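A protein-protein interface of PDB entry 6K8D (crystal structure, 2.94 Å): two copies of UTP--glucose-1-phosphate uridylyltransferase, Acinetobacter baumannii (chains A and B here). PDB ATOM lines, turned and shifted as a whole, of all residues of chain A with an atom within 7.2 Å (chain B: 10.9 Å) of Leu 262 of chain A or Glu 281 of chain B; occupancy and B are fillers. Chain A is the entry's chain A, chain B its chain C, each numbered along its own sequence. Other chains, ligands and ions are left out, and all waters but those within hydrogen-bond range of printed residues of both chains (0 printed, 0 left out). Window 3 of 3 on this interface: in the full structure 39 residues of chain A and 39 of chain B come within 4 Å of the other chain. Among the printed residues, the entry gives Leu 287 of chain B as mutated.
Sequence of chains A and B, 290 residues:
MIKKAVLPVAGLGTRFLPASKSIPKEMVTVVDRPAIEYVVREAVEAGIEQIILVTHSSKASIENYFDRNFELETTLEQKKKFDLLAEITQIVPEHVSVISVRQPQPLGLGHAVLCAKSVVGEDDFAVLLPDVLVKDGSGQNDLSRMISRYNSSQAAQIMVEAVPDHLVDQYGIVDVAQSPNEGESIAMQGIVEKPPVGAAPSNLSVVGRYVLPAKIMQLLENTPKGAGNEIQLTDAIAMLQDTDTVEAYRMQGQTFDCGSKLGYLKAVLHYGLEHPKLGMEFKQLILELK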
ATOM      1  N   PHE A  16       5.823 -13.237  17.974  1.00  0.00           N
ATOM      2  CA  PHE A  16       5.277 -13.375  16.595  1.00  0.00           C
ATOM      3  C   PHE A  16       4.058 -12.471  16.378  1.00  0.00           C
ATOM      4  O   PHE A  16       3.159 -12.864  15.627  1.00  0.00           O
ATOM      5  CB  PHE A  16       4.852 -14.833  16.386  1.00  0.00           C
ATOM      6  CG  PHE A  16       5.101 -15.365  14.999  1.00  0.00           C
ATOM      7  CD1 PHE A  16       4.465 -14.804  13.899  1.00  0.00           C
ATOM      8  CD2 PHE A  16       5.985 -16.416  14.788  1.00  0.00           C
ATOM      9  CE1 PHE A  16       4.714 -15.272  12.618  1.00  0.00           C
ATOM     10  CE2 PHE A  16       6.220 -16.891  13.508  1.00  0.00           C
ATOM     11  CZ  PHE A  16       5.585 -16.318  12.427  1.00  0.00           C
ATOM     12  N   ASP A 257      13.319 -22.390  13.552  1.00  0.00           N
ATOM     13  CA  ASP A 257      12.655 -21.764  14.724  1.00  0.00           C
ATOM     14  C   ASP A 257      11.513 -20.876  14.226  1.00  0.00           C
ATOM     15  O   ASP A 257      11.796 -19.759  13.765  1.00  0.00           O
ATOM     16  CB  ASP A 257      13.651 -21.004  15.601  1.00  0.00           C
ATOM     17  CG  ASP A 257      13.067 -20.613  16.946  1.00  0.00           C
ATOM     18  OD1 ASP A 257      12.164 -19.750  16.964  1.00  0.00           O
ATOM     19  OD2 ASP A 257      13.500 -21.194  17.963  1.00  0.00           O
ATOM     20  N   CYS A 258      10.270 -21.352  14.338  1.00  0.00           N
ATOM     21  CA  CYS A 258       9.046 -20.575  14.007  1.00  0.00           C
ATOM     22  C   CYS A 258       8.606 -19.738  15.208  1.00  0.00           C
ATOM     23  O   CYS A 258       7.454 -19.267  15.202  1.00  0.00           O
ATOM     24  CB  CYS A 258       7.930 -21.492  13.535  1.00  0.00           C
ATOM     25  SG  CYS A 258       8.472 -22.502  12.140  1.00  0.00           S
ATOM     26  N   GLY A 259       9.497 -19.553  16.186  1.00  0.00           N
ATOM     27  CA  GLY A 259       9.397 -18.485  17.197  1.00  0.00           C
ATOM     28  C   GLY A 259       9.694 -17.138  16.572  1.00  0.00           C
ATOM     29  O   GLY A 259       8.773 -16.294  16.493  1.00  0.00           O
ATOM     30  N   SER A 260      10.931 -16.957  16.106  1.00  0.00           N
ATOM     31  CA  SER A 260      11.378 -15.762  15.340  1.00  0.00           C
ATOM     32  C   SER A 260      10.628 -15.693  14.000  1.00  0.00           C
ATOM     33  O   SER A 260      10.628 -16.717  13.280  1.00  0.00           O
ATOM     34  CB  SER A 260      12.873 -15.776  15.135  1.00  0.00           C
ATOM     35  OG  SER A 260      13.255 -16.776  14.203  1.00  0.00           O
ATOM     36  N   LYS A 261      10.029 -14.531  13.687  1.00  0.00           N
ATOM     37  CA  LYS A 261       9.349 -14.225  12.390  1.00  0.00           C
ATOM     38  C   LYS A 261      10.280 -14.564  11.218  1.00  0.00           C
ATOM     39  O   LYS A 261       9.784 -15.112  10.205  1.00  0.00           O
ATOM     40  CB  LYS A 261       8.961 -12.747  12.275  1.00  0.00           C
ATOM     41  CG  LYS A 261       8.174 -12.187  13.449  1.00  0.00           C
ATOM     42  CD  LYS A 261       7.231 -11.086  13.056  1.00  0.00           C
ATOM     43  CE  LYS A 261       6.924 -10.133  14.188  1.00  0.00           C
ATOM     44  NZ  LYS A 261       6.149  -8.970  13.697  1.00  0.00           N
ATOM     45  N   LEU A 262      11.567 -14.229  11.358  1.00  0.00           N
ATOM     46  CA  LEU A 262      12.635 -14.498  10.358  1.00  0.00           C
ATOM     47  C   LEU A 262      12.799 -16.016  10.189  1.00  0.00           C
ATOM     48  O   LEU A 262      12.724 -16.496   9.043  1.00  0.00           O
ATOM     49  CB  LEU A 262      13.930 -13.830  10.831  1.00  0.00           C
ATOM     50  CG  LEU A 262      15.065 -13.814   9.808  1.00  0.00           C
ATOM     51  CD1 LEU A 262      14.784 -12.800   8.710  1.00  0.00           C
ATOM     52  CD2 LEU A 262      16.405 -13.525  10.478  1.00  0.00           C
ATOM     53  N   GLY A 263      12.989 -16.741  11.294  1.00  0.00           N
ATOM     54  CA  GLY A 263      13.110 -18.212  11.315  1.00  0.00           C
ATOM     55  C   GLY A 263      11.911 -18.900  10.679  1.00  0.00           C
ATOM     56  O   GLY A 263      12.123 -19.939  10.036  1.00  0.00           O
ATOM     57  N   TYR A 264      10.702 -18.355  10.864  1.00  0.00           N
ATOM     58  CA  TYR A 264       9.442 -18.800  10.206  1.00  0.00           C
ATOM     59  C   TYR A 264       9.594 -18.674   8.683  1.00  0.00           C
ATOM     60  O   TYR A 264       9.410 -19.697   7.977  1.00  0.00           O
ATOM     61  CB  TYR A 264       8.237 -18.024  10.756  1.00  0.00           C
ATOM     62  CG  TYR A 264       7.028 -17.937   9.855  1.00  0.00           C
ATOM     63  CD1 TYR A 264       6.888 -16.898   8.952  1.00  0.00           C
ATOM     64  CD2 TYR A 264       5.993 -18.863   9.923  1.00  0.00           C
ATOM     65  CE1 TYR A 264       5.774 -16.794   8.128  1.00  0.00           C
ATOM     66  CE2 TYR A 264       4.877 -18.778   9.099  1.00  0.00           C
ATOM     67  CZ  TYR A 264       4.763 -17.735   8.197  1.00  0.00           C
ATOM     68  OH  TYR A 264       3.691 -17.611   7.359  1.00  0.00           O
ATOM     69  N   LEU A 265       9.944 -17.480   8.185  1.00  0.00           N
ATOM     70  CA  LEU A 265      10.093 -17.220   6.721  1.00  0.00           C
ATOM     71  C   LEU A 265      11.107 -18.208   6.131  1.00  0.00           C
ATOM     72  O   LEU A 265      10.948 -18.563   4.957  1.00  0.00           O
ATOM     73  CB  LEU A 265      10.533 -15.778   6.448  1.00  0.00           C
ATOM     74  CG  LEU A 265       9.605 -14.664   6.947  1.00  0.00           C
ATOM     75  CD1 LEU A 265      10.291 -13.312   6.822  1.00  0.00           C
ATOM     76  CD2 LEU A 265       8.277 -14.642   6.207  1.00  0.00           C
ATOM     77  N   LYS A 266      12.098 -18.644   6.912  1.00  0.00           N
ATOM     78  CA  LYS A 266      13.095 -19.656   6.467  1.00  0.00           C
ATOM     79  C   LYS A 266      12.398 -21.008   6.276  1.00  0.00           C
ATOM     80  O   LYS A 266      12.716 -21.704   5.295  1.00  0.00           O
ATOM     81  CB  LYS A 266      14.253 -19.785   7.458  1.00  0.00           C
ATOM     82  CG  LYS A 266      15.478 -20.527   6.933  1.00  0.00           C
ATOM     83  CD  LYS A 266      16.308 -21.143   8.045  1.00  0.00           C
ATOM     84  CE  LYS A 266      17.779 -20.786   7.998  1.00  0.00           C
ATOM     85  NZ  LYS A 266      18.509 -21.590   6.989  1.00  0.00           N
ATOM     86  N   ALA A 267      11.491 -21.364   7.188  1.00  0.00           N
ATOM     87  CA  ALA A 267      10.771 -22.656   7.186  1.00  0.00           C
ATOM     88  C   ALA A 267       9.811 -22.681   5.998  1.00  0.00           C
ATOM     89  O   ALA A 267       9.671 -23.756   5.408  1.00  0.00           O
ATOM     90  CB  ALA A 267      10.046 -22.870   8.490  1.00  0.00           C
ATOM     91  N   VAL A 268       9.188 -21.547   5.663  1.00  0.00           N
ATOM     92  CA  VAL A 268       8.305 -21.448   4.466  1.00  0.00           C
ATOM     93  C   VAL A 268       9.143 -21.799   3.241  1.00  0.00           C
ATOM     94  O   VAL A 268       8.749 -22.722   2.526  1.00  0.00           O
ATOM     95  CB  VAL A 268       7.654 -20.065   4.291  1.00  0.00           C
ATOM     96  CG1 VAL A 268       6.988 -19.938   2.928  1.00  0.00           C
ATOM     97  CG2 VAL A 268       6.663 -19.760   5.404  1.00  0.00           C
ATOM     98  N   VAL B  31       3.594 -13.215   5.361  1.00  0.00           N
ATOM     99  CA  VAL B  31       4.862 -12.711   5.975  1.00  0.00           C
ATOM    100  C   VAL B  31       4.730 -12.787   7.501  1.00  0.00           C
ATOM    101  O   VAL B  31       5.369 -13.678   8.090  1.00  0.00           O
ATOM    102  CB  VAL B  31       5.235 -11.275   5.539  1.00  0.00           C
ATOM    103  CG1 VAL B  31       6.685 -10.971   5.879  1.00  0.00           C
ATOM    104  CG2 VAL B  31       4.974 -11.000   4.064  1.00  0.00           C
ATOM    105  N   ASP B  32       3.940 -11.888   8.106  1.00  0.00           N
ATOM    106  CA  ASP B  32       3.888 -11.695   9.581  1.00  0.00           C
ATOM    107  C   ASP B  32       2.553 -11.096  10.036  1.00  0.00           C
ATOM    108  O   ASP B  32       2.546 -10.504  11.118  1.00  0.00           O
ATOM    109  CB  ASP B  32       5.029 -10.785  10.053  1.00  0.00           C
ATOM    110  CG  ASP B  32       4.951  -9.342   9.560  1.00  0.00           C
ATOM    111  OD1 ASP B  32       4.096  -9.045   8.704  1.00  0.00           O
ATOM    112  OD2 ASP B  32       5.751  -8.521  10.038  1.00  0.00           O
ATOM    113  N   ARG B  33       1.464 -11.256   9.282  1.00  0.00           N
ATOM    114  CA  ARG B  33       0.181 -10.571   9.598  1.00  0.00           C
ATOM    115  C   ARG B  33      -0.932 -11.147   8.738  1.00  0.00           C
ATOM    116  O   ARG B  33      -0.691 -11.558   7.611  1.00  0.00           O
ATOM    117  CB  ARG B  33       0.324  -9.067   9.360  1.00  0.00           C
ATOM    118  CG  ARG B  33       0.793  -8.720   7.955  1.00  0.00           C
ATOM    119  CD  ARG B  33       1.803  -7.588   7.872  1.00  0.00           C
ATOM    120  NE  ARG B  33       1.478  -6.466   8.743  1.00  0.00           N
ATOM    121  CZ  ARG B  33       2.181  -6.073   9.802  1.00  0.00           C
ATOM    122  NH1 ARG B  33       1.756  -5.042  10.507  1.00  0.00           N
ATOM    123  NH2 ARG B  33       3.291  -6.693  10.162  1.00  0.00           N
ATOM    124  N   VAL B 268       3.469 -13.821  -0.241  1.00  0.00           N
ATOM    125  CA  VAL B 268       4.426 -14.044   0.892  1.00  0.00           C
ATOM    126  C   VAL B 268       5.872 -13.817   0.415  1.00  0.00           C
ATOM    127  O   VAL B 268       6.743 -13.573   1.282  1.00  0.00           O
ATOM    128  CB  VAL B 268       4.241 -15.446   1.514  1.00  0.00           C
ATOM    129  CG1 VAL B 268       5.369 -15.830   2.466  1.00  0.00           C
ATOM    130  CG2 VAL B 268       2.892 -15.566   2.209  1.00  0.00           C
ATOM    131  N   LEU B 269       6.129 -13.896  -0.899  1.00  0.00           N
ATOM    132  CA  LEU B 269       7.436 -13.515  -1.501  1.00  0.00           C
ATOM    133  C   LEU B 269       7.477 -11.996  -1.696  1.00  0.00           C
ATOM    134  O   LEU B 269       8.418 -11.377  -1.177  1.00  0.00           O
ATOM    135  CB  LEU B 269       7.659 -14.253  -2.824  1.00  0.00           C
ATOM    136  CG  LEU B 269       7.809 -15.769  -2.717  1.00  0.00           C
ATOM    137  CD1 LEU B 269       7.971 -16.381  -4.090  1.00  0.00           C
ATOM    138  CD2 LEU B 269       8.976 -16.170  -1.829  1.00  0.00           C
ATOM    139  N   TYR B 271       5.384  -9.107  -0.826  1.00  0.00           N
ATOM    140  CA  TYR B 271       5.184  -8.380   0.452  1.00  0.00           C
ATOM    141  C   TYR B 271       6.363  -8.668   1.387  1.00  0.00           C
ATOM    142  O   TYR B 271       6.797  -7.753   2.102  1.00  0.00           O
ATOM    143  CB  TYR B 271       3.856  -8.797   1.072  1.00  0.00           C
ATOM    144  CG  TYR B 271       2.635  -8.186   0.431  1.00  0.00           C
ATOM    145  CD1 TYR B 271       2.298  -6.869   0.689  1.00  0.00           C
ATOM    146  CD2 TYR B 271       1.781  -8.919  -0.377  1.00  0.00           C
ATOM    147  CE1 TYR B 271       1.164  -6.285   0.156  1.00  0.00           C
ATOM    148  CE2 TYR B 271       0.634  -8.350  -0.913  1.00  0.00           C
ATOM    149  CZ  TYR B 271       0.322  -7.025  -0.647  1.00  0.00           C
ATOM    150  OH  TYR B 271      -0.790  -6.413  -1.161  1.00  0.00           O
ATOM    151  N   GLY B 272       6.879  -9.899   1.339  1.00  0.00           N
ATOM    152  CA  GLY B 272       8.058 -10.363   2.102  1.00  0.00           C
ATOM    153  C   GLY B 272       9.354  -9.617   1.793  1.00  0.00           C
ATOM    154  O   GLY B 272      10.089  -9.334   2.753  1.00  0.00           O
ATOM    155  N   LEU B 273       9.676  -9.381   0.511  1.00  0.00           N
ATOM    156  CA  LEU B 273      10.925  -8.689   0.061  1.00  0.00           C
ATOM    157  C   LEU B 273      10.849  -7.194   0.399  1.00  0.00           C
ATOM    158  O   LEU B 273      11.873  -6.624   0.840  1.00  0.00           O
ATOM    159  CB  LEU B 273      11.112  -8.882  -1.446  1.00  0.00           C
ATOM    160  CG  LEU B 273      11.607 -10.260  -1.875  1.00  0.00           C
ATOM    161  CD1 LEU B 273      12.904 -10.606  -1.169  1.00  0.00           C
ATOM    162  N   GLU B 274       9.672  -6.595   0.203  1.00  0.00           N
ATOM    163  CA  GLU B 274       9.374  -5.170   0.494  1.00  0.00           C
ATOM    164  C   GLU B 274       8.889  -5.018   1.939  1.00  0.00           C
ATOM    165  O   GLU B 274       8.149  -4.050   2.216  1.00  0.00           O
ATOM    166  CB  GLU B 274       8.312  -4.647  -0.474  1.00  0.00           C
ATOM    167  CG  GLU B 274       8.806  -4.542  -1.902  1.00  0.00           C
ATOM    168  CD  GLU B 274       7.794  -3.911  -2.833  1.00  0.00           C
ATOM    169  OE1 GLU B 274       6.797  -3.335  -2.334  1.00  0.00           O
ATOM    170  OE2 GLU B 274       7.995  -4.012  -4.053  1.00  0.00           O
ATOM    171  N   HIS B 275       9.279  -5.927   2.832  1.00  0.00           N
ATOM    172  CA  HIS B 275       9.025  -5.775   4.288  1.00  0.00           C
ATOM    173  C   HIS B 275      10.048  -4.790   4.847  1.00  0.00           C
ATOM    174  O   HIS B 275      11.229  -4.854   4.487  1.00  0.00           O
ATOM    175  CB  HIS B 275       9.037  -7.121   5.026  1.00  0.00           C
ATOM    176  CG  HIS B 275       8.372  -7.066   6.361  1.00  0.00           C
ATOM    177  ND1 HIS B 275       9.067  -7.213   7.547  1.00  0.00           N
ATOM    178  CD2 HIS B 275       7.079  -6.863   6.702  1.00  0.00           C
ATOM    179  CE1 HIS B 275       8.229  -7.111   8.558  1.00  0.00           C
ATOM    180  NE2 HIS B 275       7.001  -6.897   8.068  1.00  0.00           N
ATOM    181  N   PRO B 276       9.600  -3.817   5.682  1.00  0.00           N
ATOM    182  CA  PRO B 276      10.512  -2.967   6.458  1.00  0.00           C
ATOM    183  C   PRO B 276      11.632  -3.765   7.162  1.00  0.00           C
ATOM    184  O   PRO B 276      12.750  -3.838   6.612  1.00  0.00           O
ATOM    185  CB  PRO B 276       9.608  -2.239   7.480  1.00  0.00           C
ATOM    186  CG  PRO B 276       8.162  -2.489   7.036  1.00  0.00           C
ATOM    187  CD  PRO B 276       8.188  -3.436   5.853  1.00  0.00           C
ATOM    188  N   LYS B 277      11.291  -4.399   8.297  1.00  0.00           N
ATOM    189  CA  LYS B 277      12.228  -5.007   9.281  1.00  0.00           C
ATOM    190  C   LYS B 277      12.831  -6.312   8.755  1.00  0.00           C
ATOM    191  O   LYS B 277      13.876  -6.675   9.296  1.00  0.00           O
ATOM    192  CB  LYS B 277      11.508  -5.306  10.598  1.00  0.00           C
ATOM    193  N   LEU B 278      12.202  -6.991   7.780  1.00  0.00           N
ATOM    194  CA  LEU B 278      12.587  -8.366   7.325  1.00  0.00           C
ATOM    195  C   LEU B 278      13.060  -8.377   5.867  1.00  0.00           C
ATOM    196  O   LEU B 278      13.775  -9.348   5.504  1.00  0.00           O
ATOM    197  CB  LEU B 278      11.403  -9.335   7.465  1.00  0.00           C
ATOM    198  CG  LEU B 278      11.237 -10.120   8.773  1.00  0.00           C
ATOM    199  CD1 LEU B 278      12.473 -10.062   9.669  1.00  0.00           C
ATOM    200  CD2 LEU B 278      10.008  -9.643   9.525  1.00  0.00           C
ATOM    201  N   GLY B 279      12.638  -7.399   5.057  1.00  0.00           N
ATOM    202  CA  GLY B 279      12.956  -7.348   3.616  1.00  0.00           C
ATOM    203  C   GLY B 279      14.402  -7.740   3.369  1.00  0.00           C
ATOM    204  O   GLY B 279      14.633  -8.713   2.612  1.00  0.00           O
ATOM    205  N   MET B 280      15.322  -7.047   4.052  1.00  0.00           N
ATOM    206  CA  MET B 280      16.795  -7.091   3.834  1.00  0.00           C
ATOM    207  C   MET B 280      17.319  -8.512   4.095  1.00  0.00           C
ATOM    208  O   MET B 280      18.142  -9.002   3.298  1.00  0.00           O
ATOM    209  CB  MET B 280      17.525  -6.108   4.764  1.00  0.00           C
ATOM    210  CG  MET B 280      17.040  -4.649   4.701  1.00  0.00           C
ATOM    211  SD  MET B 280      17.248  -3.792   3.105  1.00  0.00           S
ATOM    212  CE  MET B 280      18.881  -4.352   2.619  1.00  0.00           C
ATOM    213  N   GLU B 281      16.862  -9.137   5.183  1.00  0.00           N
ATOM    214  CA  GLU B 281      17.361 -10.455   5.664  1.00  0.00           C
ATOM    215  C   GLU B 281      16.608 -11.575   4.938  1.00  0.00           C
ATOM    216  O   GLU B 281      17.200 -12.658   4.763  1.00  0.00           O
ATOM    217  CB  GLU B 281      17.206 -10.605   7.182  1.00  0.00           C
ATOM    218  CG  GLU B 281      18.102  -9.688   8.003  1.00  0.00           C
ATOM    219  CD  GLU B 281      17.691  -8.225   7.993  1.00  0.00           C
ATOM    220  OE1 GLU B 281      16.498  -7.943   7.734  1.00  0.00           O
ATOM    221  OE2 GLU B 281      18.568  -7.366   8.223  1.00  0.00           O
ATOM    222  N   PHE B 282      15.347 -11.335   4.555  1.00  0.00           N
ATOM    223  CA  PHE B 282      14.533 -12.286   3.751  1.00  0.00           C
ATOM    224  C   PHE B 282      15.172 -12.402   2.366  1.00  0.00           C
ATOM    225  O   PHE B 282      15.344 -13.538   1.869  1.00  0.00           O
ATOM    226  CB  PHE B 282      13.069 -11.842   3.682  1.00  0.00           C
ATOM    227  CG  PHE B 282      12.157 -12.778   2.925  1.00  0.00           C
ATOM    228  CD1 PHE B 282      12.203 -14.150   3.137  1.00  0.00           C
ATOM    229  CD2 PHE B 282      11.242 -12.282   2.007  1.00  0.00           C
ATOM    230  CE1 PHE B 282      11.364 -15.003   2.438  1.00  0.00           C
ATOM    231  CE2 PHE B 282      10.403 -13.135   1.307  1.00  0.00           C
ATOM    232  CZ  PHE B 282      10.468 -14.494   1.523  1.00  0.00           C
ATOM    233  N   LYS B 283      15.534 -11.246   1.794  1.00  0.00           N
ATOM    234  CA  LYS B 283      16.300 -11.126   0.523  1.00  0.00           C
ATOM    235  C   LYS B 283      17.574 -11.969   0.656  1.00  0.00           C
ATOM    236  O   LYS B 283      17.961 -12.630  -0.326  1.00  0.00           O
ATOM    237  CB  LYS B 283      16.587  -9.649   0.208  1.00  0.00           C
ATOM    238  CG  LYS B 283      16.760  -9.339  -1.272  1.00  0.00           C
ATOM    239  CD  LYS B 283      17.608  -8.118  -1.575  1.00  0.00           C
ATOM    240  CE  LYS B 283      18.178  -8.135  -2.981  1.00  0.00           C
ATOM    241  NZ  LYS B 283      18.227  -6.782  -3.588  1.00  0.00           N
ATOM    242  N   GLN B 284      18.171 -11.965   1.852  1.00  0.00           N
ATOM    243  CA  GLN B 284      19.389 -12.741   2.212  1.00  0.00           C
ATOM    244  C   GLN B 284      19.092 -14.248   2.151  1.00  0.00           C
ATOM    245  O   GLN B 284      19.915 -14.990   1.565  1.00  0.00           O
ATOM    246  CB  GLN B 284      19.872 -12.351   3.614  1.00  0.00           C
ATOM    247  CG  GLN B 284      21.374 -12.139   3.715  1.00  0.00           C
ATOM    248  CD  GLN B 284      21.770 -10.756   3.262  1.00  0.00           C
ATOM    249  OE1 GLN B 284      21.109 -10.141   2.425  1.00  0.00           O
ATOM    250  NE2 GLN B 284      22.859 -10.251   3.821  1.00  0.00           N
ATOM    251  N   LEU B 285      17.969 -14.674   2.742  1.00  0.00           N
ATOM    252  CA  LEU B 285      17.584 -16.105   2.907  1.00  0.00           C
ATOM    253  C   LEU B 285      17.332 -16.752   1.538  1.00  0.00           C
ATOM    254  O   LEU B 285      17.748 -17.927   1.359  1.00  0.00           O
ATOM    255  CB  LEU B 285      16.348 -16.193   3.809  1.00  0.00           C
ATOM    256  CG  LEU B 285      16.615 -15.981   5.300  1.00  0.00           C
ATOM    257  CD1 LEU B 285      15.349 -15.567   6.031  1.00  0.00           C
ATOM    258  CD2 LEU B 285      17.204 -17.233   5.932  1.00  0.00           C
ATOM    259  N   ILE B 286      16.695 -16.015   0.616  1.00  0.00           N
ATOM    260  CA  ILE B 286      16.351 -16.477  -0.766  1.00  0.00           C
ATOM    261  C   ILE B 286      17.642 -16.797  -1.523  1.00  0.00           C
ATOM    262  O   ILE B 286      17.632 -17.740  -2.349  1.00  0.00           O
ATOM    263  CB  ILE B 286      15.515 -15.419  -1.510  1.00  0.00           C
ATOM    264  CG1 ILE B 286      14.117 -15.288  -0.902  1.00  0.00           C
ATOM    265  CD1 ILE B 286      13.537 -13.901  -0.999  1.00  0.00           C
ATOM    266  N   LEU B 287      18.704 -16.035  -1.244  1.00  0.00           N
ATOM    267  CA  LEU B 287      20.037 -16.185  -1.887  1.00  0.00           C
ATOM    268  C   LEU B 287      20.773 -17.395  -1.297  1.00  0.00           C
ATOM    269  O   LEU B 287      21.638 -17.937  -1.996  1.00  0.00           O
ATOM    270  CB  LEU B 287      20.834 -14.892  -1.689  1.00  0.00           C
ATOM    271  CG  LEU B 287      20.138 -13.609  -2.149  1.00  0.00           C
ATOM    272  CD1 LEU B 287      20.158 -13.494  -3.667  1.00  0.00           C
ATOM    273  N   GLU B 288      20.418 -17.822  -0.080  1.00  0.00           N
ATOM    274  CA  GLU B 288      21.098 -18.920   0.659  1.00  0.00           C
ATOM    275  C   GLU B 288      20.479 -20.287   0.319  1.00  0.00           C
ATOM    276  O   GLU B 288      20.783 -21.248   1.048  1.00  0.00           O
ATOM    277  CB  GLU B 288      21.015 -18.650   2.162  1.00  0.00           C
ATOM    278  CG  GLU B 288      21.747 -17.390   2.595  1.00  0.00           C
ATOM    279  CD  GLU B 288      21.275 -16.786   3.910  1.00  0.00           C
ATOM    280  OE1 GLU B 288      20.516 -17.462   4.629  1.00  0.00           O
ATOM    281  OE2 GLU B 288      21.667 -15.639   4.218  1.00  0.00           O
ATOM    282  N   LEU B 289      19.690 -20.394  -0.760  1.00  0.00           N
ATOM    283  CA  LEU B 289      18.807 -21.565  -1.054  1.00  0.00           C
ATOM    284  C   LEU B 289      19.580 -22.725  -1.710  1.00  0.00           C
ATOM    285  O   LEU B 289      19.090 -23.868  -1.614  1.00  0.00           O
ATOM    286  CB  LEU B 289      17.648 -21.114  -1.952  1.00  0.00           C
ATOM    287  CG  LEU B 289      16.642 -20.165  -1.306  1.00  0.00           C
ATOM    288  CD2 LEU B 289      15.815 -20.896  -0.269  1.00  0.00           C
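OD2 of Asp 32 of chain B lies within salt-bridge range of NZ of Lys 261 of chain A (3.7 Å).
The backbone carbonyl oxygen of Asp 257 of chain A is in hydrogen-bond range of the backbone NH of Tyr 264 of chain A, at 3.4 Å.
The side-chain carboxylate of Asp 32 of chain B lies within salt-bridge range of the guanidinium group of Arg 33 of chain B, 2.9 Å away.
NE2 of His 275 of chain B sits at hydrogen-bond distance from OD2 of Asp 32 of chain B, at 2.8 Å.
The backbone NH (N) of Leu 278 of chain B sits at hydrogen-bond distance from a ring nitrogen (ND1) of His 275 of chain B (3.2 Å).
Among the printed residues, merely in contact across the chains: Tyr 264 of chain A with Val 31 of chain B, Leu 265 of chain A with Val 31 of chain B, Leu 262 of chain A with Glu 281 of chain B, Leu 262 of chain A with Leu 278 of chain B, Lys 266 of chain A with Leu 285 of chain B, Leu 265 of chain A with Leu 278 of chain B and Leu 262 of chain A with Leu 285 of chain B.
No residue of chain B comes within 4 Å of Ser 260 of chain A.
Of chain B, only Leu 278 (3.7 Å), Glu 281 (3.6 Å) and Leu 285 (3.9 Å) come within 4 Å of Leu 262 of chain A.
No residue of chain B comes within 4 Å of Gly 263 of chain A.
Leu 265 of chain A touches just these residues of chain B: Val 31 (3.6 Å) and Leu 278 (3.9 Å).
Of the printed residues of chain B, Lys 266 of chain A touches Leu 285.
Printed residues of chain A within 4 Å of Leu 278 of chain B: Leu 262 and Leu 265.
Of chain A, only Leu 262 comes within 4 Å of Glu 281 of chain B.
The nearest residue of chain A that does not touch Glu 281 of chain B is Leu 265 of chain A (6.8 Å).
The nearest printed residue of chain B that does not touch Lys 266 of chain A is Glu 288 of chain B (5.2 Å).
Of the 13 printed residues of chain A, 5 touch a printed residue of chain B.
Hydrophobic or aromatic side chains of chain A that line the printed part of chain B: Leu 262, Tyr 264 and Leu 265.
Printed residues of chain B that touch a printed residue of chain A: Val 31, Asp 32, Leu 278, Glu 281 and Leu 285.
Hydrophobic or aromatic side chains of chain B that line the printed part of chain A: Leu 278 and Leu 285.
Position printed for both chains: 268.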
